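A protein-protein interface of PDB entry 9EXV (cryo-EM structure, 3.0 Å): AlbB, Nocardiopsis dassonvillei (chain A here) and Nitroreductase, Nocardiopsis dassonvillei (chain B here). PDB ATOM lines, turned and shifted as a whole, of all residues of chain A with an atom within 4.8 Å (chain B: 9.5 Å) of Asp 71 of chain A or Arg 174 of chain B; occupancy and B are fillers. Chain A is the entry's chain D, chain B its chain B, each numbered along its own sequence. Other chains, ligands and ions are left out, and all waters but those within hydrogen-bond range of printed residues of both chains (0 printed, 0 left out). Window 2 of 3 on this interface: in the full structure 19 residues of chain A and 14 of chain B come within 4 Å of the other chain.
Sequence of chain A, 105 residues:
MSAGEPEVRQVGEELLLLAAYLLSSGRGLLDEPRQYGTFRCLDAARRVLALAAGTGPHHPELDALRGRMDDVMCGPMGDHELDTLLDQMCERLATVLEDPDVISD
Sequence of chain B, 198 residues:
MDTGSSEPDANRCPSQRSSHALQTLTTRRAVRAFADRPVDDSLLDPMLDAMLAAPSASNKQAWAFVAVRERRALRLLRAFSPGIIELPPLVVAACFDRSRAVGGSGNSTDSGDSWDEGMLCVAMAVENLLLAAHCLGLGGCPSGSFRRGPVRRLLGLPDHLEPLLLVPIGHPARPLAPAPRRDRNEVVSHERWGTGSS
O of Gly 75 of chain A sits at hydrogen-bond distance from NH1 of Arg 32 of chain B, at 3.4 Å.
The side-chain carboxylate (OD1) of Asp 71 of chain A lies within salt-bridge range of the guanidinium group (NH2) of Arg 174 of chain B, 3.8 Å away.
NH1 of Arg 174 of chain B lies within hydrogen-bond range of O of Cys 74 of chain A (3.5 Å).
Of the 19 printed residues of chain B, 3 touch a printed residue of chain A.
Printed residues of chain B that touch a printed residue of chain A: Arg 32, Arg 174 and Ala 177.
Hydrophobic or aromatic side chains of chain B within 4 Å of the printed part of chain A: Ala 177.
Hydrophobic or aromatic side chains of chain A within 4 Å of the printed part of chain B: Pro 76.
Along chain A the printed residues that touch a printed residue of chain B span positions 71 to 76.
Asp 71 of chain A touches just one residue of chain B: Arg 174.
No residue of chain B comes within 4 Å of Asp 70 of chain A.
No residue of chain B comes within 4 Å of Val 72 of chain A.
Gly 75 of chain A touches just these residues of chain B: Arg 32 (3.4 Å) and Arg 174 (3.1 Å).
Printed residues of chain B within 4 Å of Pro 76 of chain A: Ala 177.
Of the printed residues of chain B, Met 73 of chain A touches Arg 32 (3.5 Å).
Printed residues of chain A within 4 Å of Arg 32 of chain B: Met 73, Cys 74 and Gly 75.
Pro 175 of chain B touches none of the printed residues of chain A.
Arg 68 of chain A touches none of the printed residues of chain B.
The nearest printed residue of chain B that does not touch Pro 76 of chain A is Arg 174 of chain B (4.4 Å).
Met 73 of chain A touches Arg 32 of chain B (O to CD, 3.5 Å).
CB of Arg 32 of chain B touches O of Cys 74 of chain A, at 3.4 Å.
Arg 174 of chain B touches Gly 75 of chain A (NH1 to CA, 3.1 Å).
Pro 76 of chain A touches Ala 177 of chain B (CG to CB, 3.8 Å).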
ATOM      1  N   GLY A  67       9.887 -24.226 -11.606  1.00  0.00           N
ATOM      2  CA  GLY A  67      10.691 -24.075 -10.407  1.00  0.00           C
ATOM      3  C   GLY A  67      12.112 -23.637 -10.707  1.00  0.00           C
ATOM      4  O   GLY A  67      12.669 -22.785 -10.013  1.00  0.00           O
ATOM      5  N   ARG A  68      12.718 -24.219 -11.744  1.00  0.00           N
ATOM      6  CA  ARG A  68      14.065 -23.817 -12.126  1.00  0.00           C
ATOM      7  C   ARG A  68      14.101 -22.357 -12.561  1.00  0.00           C
ATOM      8  O   ARG A  68      15.010 -21.610 -12.181  1.00  0.00           O
ATOM      9  CB  ARG A  68      14.586 -24.718 -13.245  1.00  0.00           C
ATOM     10  CG  ARG A  68      16.065 -24.516 -13.566  1.00  0.00           C
ATOM     11  CD  ARG A  68      16.642 -25.656 -14.408  1.00  0.00           C
ATOM     12  NE  ARG A  68      16.034 -26.943 -14.084  1.00  0.00           N
ATOM     13  CZ  ARG A  68      16.126 -27.543 -12.905  1.00  0.00           C
ATOM     14  NH1 ARG A  68      16.807 -27.006 -11.906  1.00  0.00           N
ATOM     15  NH2 ARG A  68      15.494 -28.697 -12.715  1.00  0.00           N
ATOM     16  N   MET A  69      13.121 -21.933 -13.356  1.00  0.00           N
ATOM     17  CA  MET A  69      13.071 -20.538 -13.774  1.00  0.00           C
ATOM     18  C   MET A  69      12.886 -19.614 -12.580  1.00  0.00           C
ATOM     19  O   MET A  69      13.488 -18.536 -12.520  1.00  0.00           O
ATOM     20  CB  MET A  69      11.949 -20.333 -14.792  1.00  0.00           C
ATOM     21  CG  MET A  69      12.116 -21.135 -16.067  1.00  0.00           C
ATOM     22  SD  MET A  69      10.780 -20.853 -17.240  1.00  0.00           S
ATOM     23  CE  MET A  69      10.931 -22.320 -18.249  1.00  0.00           C
ATOM     24  N   ASP A  70      12.050 -20.018 -11.622  1.00  0.00           N
ATOM     25  CA  ASP A  70      11.861 -19.222 -10.416  1.00  0.00           C
ATOM     26  C   ASP A  70      13.160 -19.094  -9.634  1.00  0.00           C
ATOM     27  O   ASP A  70      13.495 -18.009  -9.147  1.00  0.00           O
ATOM     28  CB  ASP A  70      10.768 -19.838  -9.544  1.00  0.00           C
ATOM     29  CG  ASP A  70       9.385 -19.683 -10.145  1.00  0.00           C
ATOM     30  OD1 ASP A  70       9.143 -18.668 -10.830  1.00  0.00           O
ATOM     31  OD2 ASP A  70       8.538 -20.576  -9.930  1.00  0.00           O
ATOM     32  N   ASP A  71      13.908 -20.191  -9.506  1.00  0.00           N
ATOM     33  CA  ASP A  71      15.197 -20.117  -8.830  1.00  0.00           C
ATOM     34  C   ASP A  71      16.146 -19.175  -9.559  1.00  0.00           C
ATOM     35  O   ASP A  71      16.870 -18.399  -8.926  1.00  0.00           O
ATOM     36  CB  ASP A  71      15.815 -21.509  -8.706  1.00  0.00           C
ATOM     37  CG  ASP A  71      15.177 -22.334  -7.607  1.00  0.00           C
ATOM     38  OD1 ASP A  71      14.105 -21.935  -7.106  1.00  0.00           O
ATOM     39  OD2 ASP A  71      15.754 -23.378  -7.236  1.00  0.00           O
ATOM     40  N   VAL A  72      16.156 -19.226 -10.892  1.00  0.00           N
ATOM     41  CA  VAL A  72      17.065 -18.380 -11.659  1.00  0.00           C
ATOM     42  C   VAL A  72      16.725 -16.907 -11.465  1.00  0.00           C
ATOM     43  O   VAL A  72      17.609 -16.073 -11.236  1.00  0.00           O
ATOM     44  CB  VAL A  72      17.042 -18.769 -13.149  1.00  0.00           C
ATOM     45  CG1 VAL A  72      17.758 -17.714 -13.983  1.00  0.00           C
ATOM     46  CG2 VAL A  72      17.681 -20.130 -13.352  1.00  0.00           C
ATOM     47  N   MET A  73      15.440 -16.564 -11.543  1.00  0.00           N
ATOM     48  CA  MET A  73      15.033 -15.161 -11.569  1.00  0.00           C
ATOM     49  C   MET A  73      14.769 -14.602 -10.175  1.00  0.00           C
ATOM     50  O   MET A  73      15.441 -13.665  -9.735  1.00  0.00           O
ATOM     51  CB  MET A  73      13.788 -14.996 -12.445  1.00  0.00           C
ATOM     52  CG  MET A  73      13.990 -15.412 -13.882  1.00  0.00           C
ATOM     53  SD  MET A  73      15.019 -14.258 -14.808  1.00  0.00           S
ATOM     54  CE  MET A  73      14.055 -12.758 -14.649  1.00  0.00           C
ATOM     55  N   CYS A  74      13.795 -15.175  -9.468  1.00  0.00           N
ATOM     56  CA  CYS A  74      13.413 -14.668  -8.157  1.00  0.00           C
ATOM     57  C   CYS A  74      14.519 -14.817  -7.123  1.00  0.00           C
ATOM     58  O   CYS A  74      14.423 -14.216  -6.048  1.00  0.00           O
ATOM     59  CB  CYS A  74      12.151 -15.377  -7.668  1.00  0.00           C
ATOM     60  N   GLY A  75      15.552 -15.601  -7.413  1.00  0.00           N
ATOM     61  CA  GLY A  75      16.625 -15.824  -6.476  1.00  0.00           C
ATOM     62  C   GLY A  75      17.806 -14.903  -6.683  1.00  0.00           C
ATOM     63  O   GLY A  75      17.723 -13.890  -7.387  1.00  0.00           O
ATOM     64  N   PRO A  76      18.936 -15.243  -6.064  1.00  0.00           N
ATOM     65  CA  PRO A  76      20.120 -14.386  -6.175  1.00  0.00           C
ATOM     66  C   PRO A  76      20.550 -14.226  -7.626  1.00  0.00           C
ATOM     67  O   PRO A  76      20.421 -15.141  -8.442  1.00  0.00           O
ATOM     68  CB  PRO A  76      21.181 -15.133  -5.359  1.00  0.00           C
ATOM     69  CG  PRO A  76      20.408 -16.024  -4.443  1.00  0.00           C
ATOM     70  CD  PRO A  76      19.170 -16.407  -5.194  1.00  0.00           C
ATOM     71  N   ARG B  29      18.537  -8.156   2.295  1.00  0.00           N
ATOM     72  CA  ARG B  29      18.634  -8.851   1.020  1.00  0.00           C
ATOM     73  C   ARG B  29      17.395  -8.558   0.184  1.00  0.00           C
ATOM     74  O   ARG B  29      16.277  -8.523   0.708  1.00  0.00           O
ATOM     75  CB  ARG B  29      18.790 -10.366   1.224  1.00  0.00           C
ATOM     76  CG  ARG B  29      20.029 -10.762   2.022  1.00  0.00           C
ATOM     77  CD  ARG B  29      21.303 -10.404   1.269  1.00  0.00           C
ATOM     78  NE  ARG B  29      22.423 -10.126   2.159  1.00  0.00           N
ATOM     79  CZ  ARG B  29      23.380  -9.241   1.904  1.00  0.00           C
ATOM     80  NH1 ARG B  29      23.366  -8.507   0.805  1.00  0.00           N
ATOM     81  NH2 ARG B  29      24.368  -9.083   2.780  1.00  0.00           N
ATOM     82  N   ALA B  30      17.605  -8.347  -1.112  1.00  0.00           N
ATOM     83  CA  ALA B  30      16.495  -8.066  -2.011  1.00  0.00           C
ATOM     84  C   ALA B  30      15.561  -9.265  -2.093  1.00  0.00           C
ATOM     85  O   ALA B  30      16.003 -10.416  -2.157  1.00  0.00           O
ATOM     86  CB  ALA B  30      17.017  -7.704  -3.401  1.00  0.00           C
ATOM     87  N   VAL B  31      14.260  -8.991  -2.091  1.00  0.00           N
ATOM     88  CA  VAL B  31      13.227 -10.020  -2.110  1.00  0.00           C
ATOM     89  C   VAL B  31      12.453  -9.891  -3.413  1.00  0.00           C
ATOM     90  O   VAL B  31      11.828  -8.855  -3.668  1.00  0.00           O
ATOM     91  CB  VAL B  31      12.284  -9.904  -0.903  1.00  0.00           C
ATOM     92  CG1 VAL B  31      11.182 -10.950  -0.988  1.00  0.00           C
ATOM     93  CG2 VAL B  31      13.063 -10.040   0.393  1.00  0.00           C
ATOM     94  N   ARG B  32      12.482 -10.946  -4.227  1.00  0.00           N
ATOM     95  CA  ARG B  32      11.755 -10.982  -5.487  1.00  0.00           C
ATOM     96  C   ARG B  32      10.576 -11.944  -5.473  1.00  0.00           C
ATOM     97  O   ARG B  32       9.739 -11.882  -6.380  1.00  0.00           O
ATOM     98  CB  ARG B  32      12.702 -11.355  -6.636  1.00  0.00           C
ATOM     99  CG  ARG B  32      13.838 -10.365  -6.847  1.00  0.00           C
ATOM    100  CD  ARG B  32      15.040 -11.026  -7.509  1.00  0.00           C
ATOM    101  NE  ARG B  32      16.180 -10.122  -7.596  1.00  0.00           N
ATOM    102  CZ  ARG B  32      17.202 -10.099  -6.751  1.00  0.00           C
ATOM    103  NH1 ARG B  32      17.295 -10.964  -5.756  1.00  0.00           N
ATOM    104  NH2 ARG B  32      18.155  -9.185  -6.912  1.00  0.00           N
ATOM    105  N   ALA B  33      10.490 -12.826  -4.482  1.00  0.00           N
ATOM    106  CA  ALA B  33       9.378 -13.756  -4.337  1.00  0.00           C
ATOM    107  C   ALA B  33       8.591 -13.376  -3.093  1.00  0.00           C
ATOM    108  O   ALA B  33       9.134 -13.391  -1.983  1.00  0.00           O
ATOM    109  CB  ALA B  33       9.868 -15.194  -4.246  1.00  0.00           C
ATOM    110  N   PHE B  34       7.316 -13.048  -3.277  1.00  0.00           N
ATOM    111  CA  PHE B  34       6.462 -12.562  -2.205  1.00  0.00           C
ATOM    112  C   PHE B  34       5.318 -13.539  -1.983  1.00  0.00           C
ATOM    113  O   PHE B  34       4.696 -14.002  -2.945  1.00  0.00           O
ATOM    114  CB  PHE B  34       5.915 -11.172  -2.534  1.00  0.00           C
ATOM    115  CG  PHE B  34       6.953 -10.229  -3.061  1.00  0.00           C
ATOM    116  CD1 PHE B  34       7.797  -9.555  -2.196  1.00  0.00           C
ATOM    117  CD2 PHE B  34       7.093 -10.022  -4.423  1.00  0.00           C
ATOM    118  CE1 PHE B  34       8.758  -8.688  -2.678  1.00  0.00           C
ATOM    119  CE2 PHE B  34       8.051  -9.157  -4.912  1.00  0.00           C
ATOM    120  CZ  PHE B  34       8.883  -8.489  -4.039  1.00  0.00           C
ATOM    121  N   ALA B  35       5.049 -13.851  -0.720  1.00  0.00           N
ATOM    122  CA  ALA B  35       3.905 -14.679  -0.386  1.00  0.00           C
ATOM    123  C   ALA B  35       2.613 -13.951  -0.737  1.00  0.00           C
ATOM    124  O   ALA B  35       2.583 -12.729  -0.915  1.00  0.00           O
ATOM    125  CB  ALA B  35       3.918 -15.044   1.098  1.00  0.00           C
ATOM    126  N   ILE B  85       9.342  -8.609 -10.402  1.00  0.00           N
ATOM    127  CA  ILE B  85       9.423 -10.014 -10.788  1.00  0.00           C
ATOM    128  C   ILE B  85       8.124 -10.752 -10.493  1.00  0.00           C
ATOM    129  O   ILE B  85       7.577 -11.440 -11.360  1.00  0.00           O
ATOM    130  CB  ILE B  85      10.626 -10.681 -10.090  1.00  0.00           C
ATOM    131  CG1 ILE B  85      11.934 -10.008 -10.518  1.00  0.00           C
ATOM    132  CG2 ILE B  85      10.666 -12.170 -10.392  1.00  0.00           C
ATOM    133  CD1 ILE B  85      12.294 -10.215 -11.980  1.00  0.00           C
ATOM    134  N   GLU B  86       7.605 -10.627  -9.274  1.00  0.00           N
ATOM    135  CA  GLU B  86       6.376 -11.293  -8.872  1.00  0.00           C
ATOM    136  C   GLU B  86       5.424 -10.272  -8.264  1.00  0.00           C
ATOM    137  O   GLU B  86       5.835  -9.189  -7.839  1.00  0.00           O
ATOM    138  CB  GLU B  86       6.648 -12.430  -7.876  1.00  0.00           C
ATOM    139  CG  GLU B  86       5.438 -13.300  -7.565  1.00  0.00           C
ATOM    140  CD  GLU B  86       5.778 -14.494  -6.703  1.00  0.00           C
ATOM    141  OE1 GLU B  86       6.971 -14.673  -6.380  1.00  0.00           O
ATOM    142  OE2 GLU B  86       4.856 -15.256  -6.347  1.00  0.00           O
ATOM    143  N   GLY B 137      10.481  -7.677   9.126  1.00  0.00           N
ATOM    144  CA  GLY B 137      10.556  -9.013   8.575  1.00  0.00           C
ATOM    145  C   GLY B 137      10.138  -9.132   7.131  1.00  0.00           C
ATOM    146  O   GLY B 137      10.282 -10.214   6.546  1.00  0.00           O
ATOM    147  N   GLY B 139      10.304  -7.607   2.982  1.00  0.00           N
ATOM    148  CA  GLY B 139      11.408  -7.292   2.100  1.00  0.00           C
ATOM    149  C   GLY B 139      10.973  -6.493   0.892  1.00  0.00           C
ATOM    150  O   GLY B 139       9.887  -6.721   0.348  1.00  0.00           O
ATOM    151  N   GLY B 170       6.817  -6.908   0.326  1.00  0.00           N
ATOM    152  CA  GLY B 170       5.910  -7.929   0.811  1.00  0.00           C
ATOM    153  C   GLY B 170       6.654  -8.930   1.668  1.00  0.00           C
ATOM    154  O   GLY B 170       7.881  -8.885   1.803  1.00  0.00           O
ATOM    155  N   HIS B 171       5.884  -9.840   2.245  1.00  0.00           N
ATOM    156  CA  HIS B 171       6.457 -10.867   3.103  1.00  0.00           C
ATOM    157  C   HIS B 171       7.286 -11.842   2.275  1.00  0.00           C
ATOM    158  O   HIS B 171       6.795 -12.356   1.263  1.00  0.00           O
ATOM    159  CB  HIS B 171       5.346 -11.604   3.847  1.00  0.00           C
ATOM    160  CG  HIS B 171       4.627 -10.754   4.847  1.00  0.00           C
ATOM    161  ND1 HIS B 171       3.835  -9.686   4.485  1.00  0.00           N
ATOM    162  CD2 HIS B 171       4.590 -10.808   6.199  1.00  0.00           C
ATOM    163  CE1 HIS B 171       3.337  -9.123   5.571  1.00  0.00           C
ATOM    164  NE2 HIS B 171       3.780  -9.784   6.624  1.00  0.00           N
ATOM    165  N   PRO B 172       8.539 -12.110   2.650  1.00  0.00           N
ATOM    166  CA  PRO B 172       9.344 -13.064   1.881  1.00  0.00           C
ATOM    167  C   PRO B 172       8.717 -14.449   1.867  1.00  0.00           C
ATOM    168  O   PRO B 172       8.070 -14.877   2.826  1.00  0.00           O
ATOM    169  CB  PRO B 172      10.688 -13.072   2.620  1.00  0.00           C
ATOM    170  CG  PRO B 172      10.747 -11.764   3.312  1.00  0.00           C
ATOM    171  CD  PRO B 172       9.333 -11.426   3.686  1.00  0.00           C
ATOM    172  N   ALA B 173       8.912 -15.151   0.750  1.00  0.00           N
ATOM    173  CA  ALA B 173       8.394 -16.499   0.574  1.00  0.00           C
ATOM    174  C   ALA B 173       9.474 -17.566   0.505  1.00  0.00           C
ATOM    175  O   ALA B 173       9.180 -18.734   0.775  1.00  0.00           O
ATOM    176  CB  ALA B 173       7.537 -16.580  -0.698  1.00  0.00           C
ATOM    177  N   ARG B 174      10.702 -17.202   0.152  1.00  0.00           N
ATOM    178  CA  ARG B 174      11.808 -18.139   0.047  1.00  0.00           C
ATOM    179  C   ARG B 174      13.017 -17.605   0.795  1.00  0.00           C
ATOM    180  O   ARG B 174      13.158 -16.389   0.962  1.00  0.00           O
ATOM    181  CB  ARG B 174      12.175 -18.395  -1.423  1.00  0.00           C
ATOM    182  CG  ARG B 174      12.273 -17.141  -2.275  1.00  0.00           C
ATOM    183  CD  ARG B 174      12.199 -17.494  -3.751  1.00  0.00           C
ATOM    184  NE  ARG B 174      13.148 -18.532  -4.106  1.00  0.00           N
ATOM    185  CZ  ARG B 174      14.439 -18.318  -4.311  1.00  0.00           C
ATOM    186  NH1 ARG B 174      14.961 -17.109  -4.207  1.00  0.00           N
ATOM    187  NH2 ARG B 174      15.226 -19.345  -4.619  1.00  0.00           N
ATOM    188  N   PRO B 175      13.902 -18.486   1.264  1.00  0.00           N
ATOM    189  CA  PRO B 175      15.082 -18.016   1.998  1.00  0.00           C
ATOM    190  C   PRO B 175      15.939 -17.094   1.142  1.00  0.00           C
ATOM    191  O   PRO B 175      16.060 -17.272  -0.071  1.00  0.00           O
ATOM    192  CB  PRO B 175      15.825 -19.312   2.343  1.00  0.00           C
ATOM    193  CG  PRO B 175      14.783 -20.372   2.303  1.00  0.00           C
ATOM    194  CD  PRO B 175      13.822 -19.958   1.231  1.00  0.00           C
ATOM    195  N   LEU B 176      16.530 -16.099   1.793  1.00  0.00           N
ATOM    196  CA  LEU B 176      17.349 -15.097   1.125  1.00  0.00           C
ATOM    197  C   LEU B 176      18.824 -15.461   1.237  1.00  0.00           C
ATOM    198  O   LEU B 176      19.292 -15.885   2.296  1.00  0.00           O
ATOM    199  CB  LEU B 176      17.102 -13.712   1.722  1.00  0.00           C
ATOM    200  CG  LEU B 176      15.677 -13.188   1.527  1.00  0.00           C
ATOM    201  CD1 LEU B 176      15.441 -11.916   2.328  1.00  0.00           C
ATOM    202  CD2 LEU B 176      15.395 -12.955   0.049  1.00  0.00           C
ATOM    203  N   ALA B 177      19.550 -15.295   0.133  1.00  0.00           N
ATOM    204  CA  ALA B 177      20.971 -15.588   0.085  1.00  0.00           C
ATOM    205  C   ALA B 177      21.732 -14.384  -0.453  1.00  0.00           C
ATOM    206  O   ALA B 177      21.232 -13.677  -1.335  1.00  0.00           O
ATOM    207  CB  ALA B 177      21.252 -16.816  -0.794  1.00  0.00           C
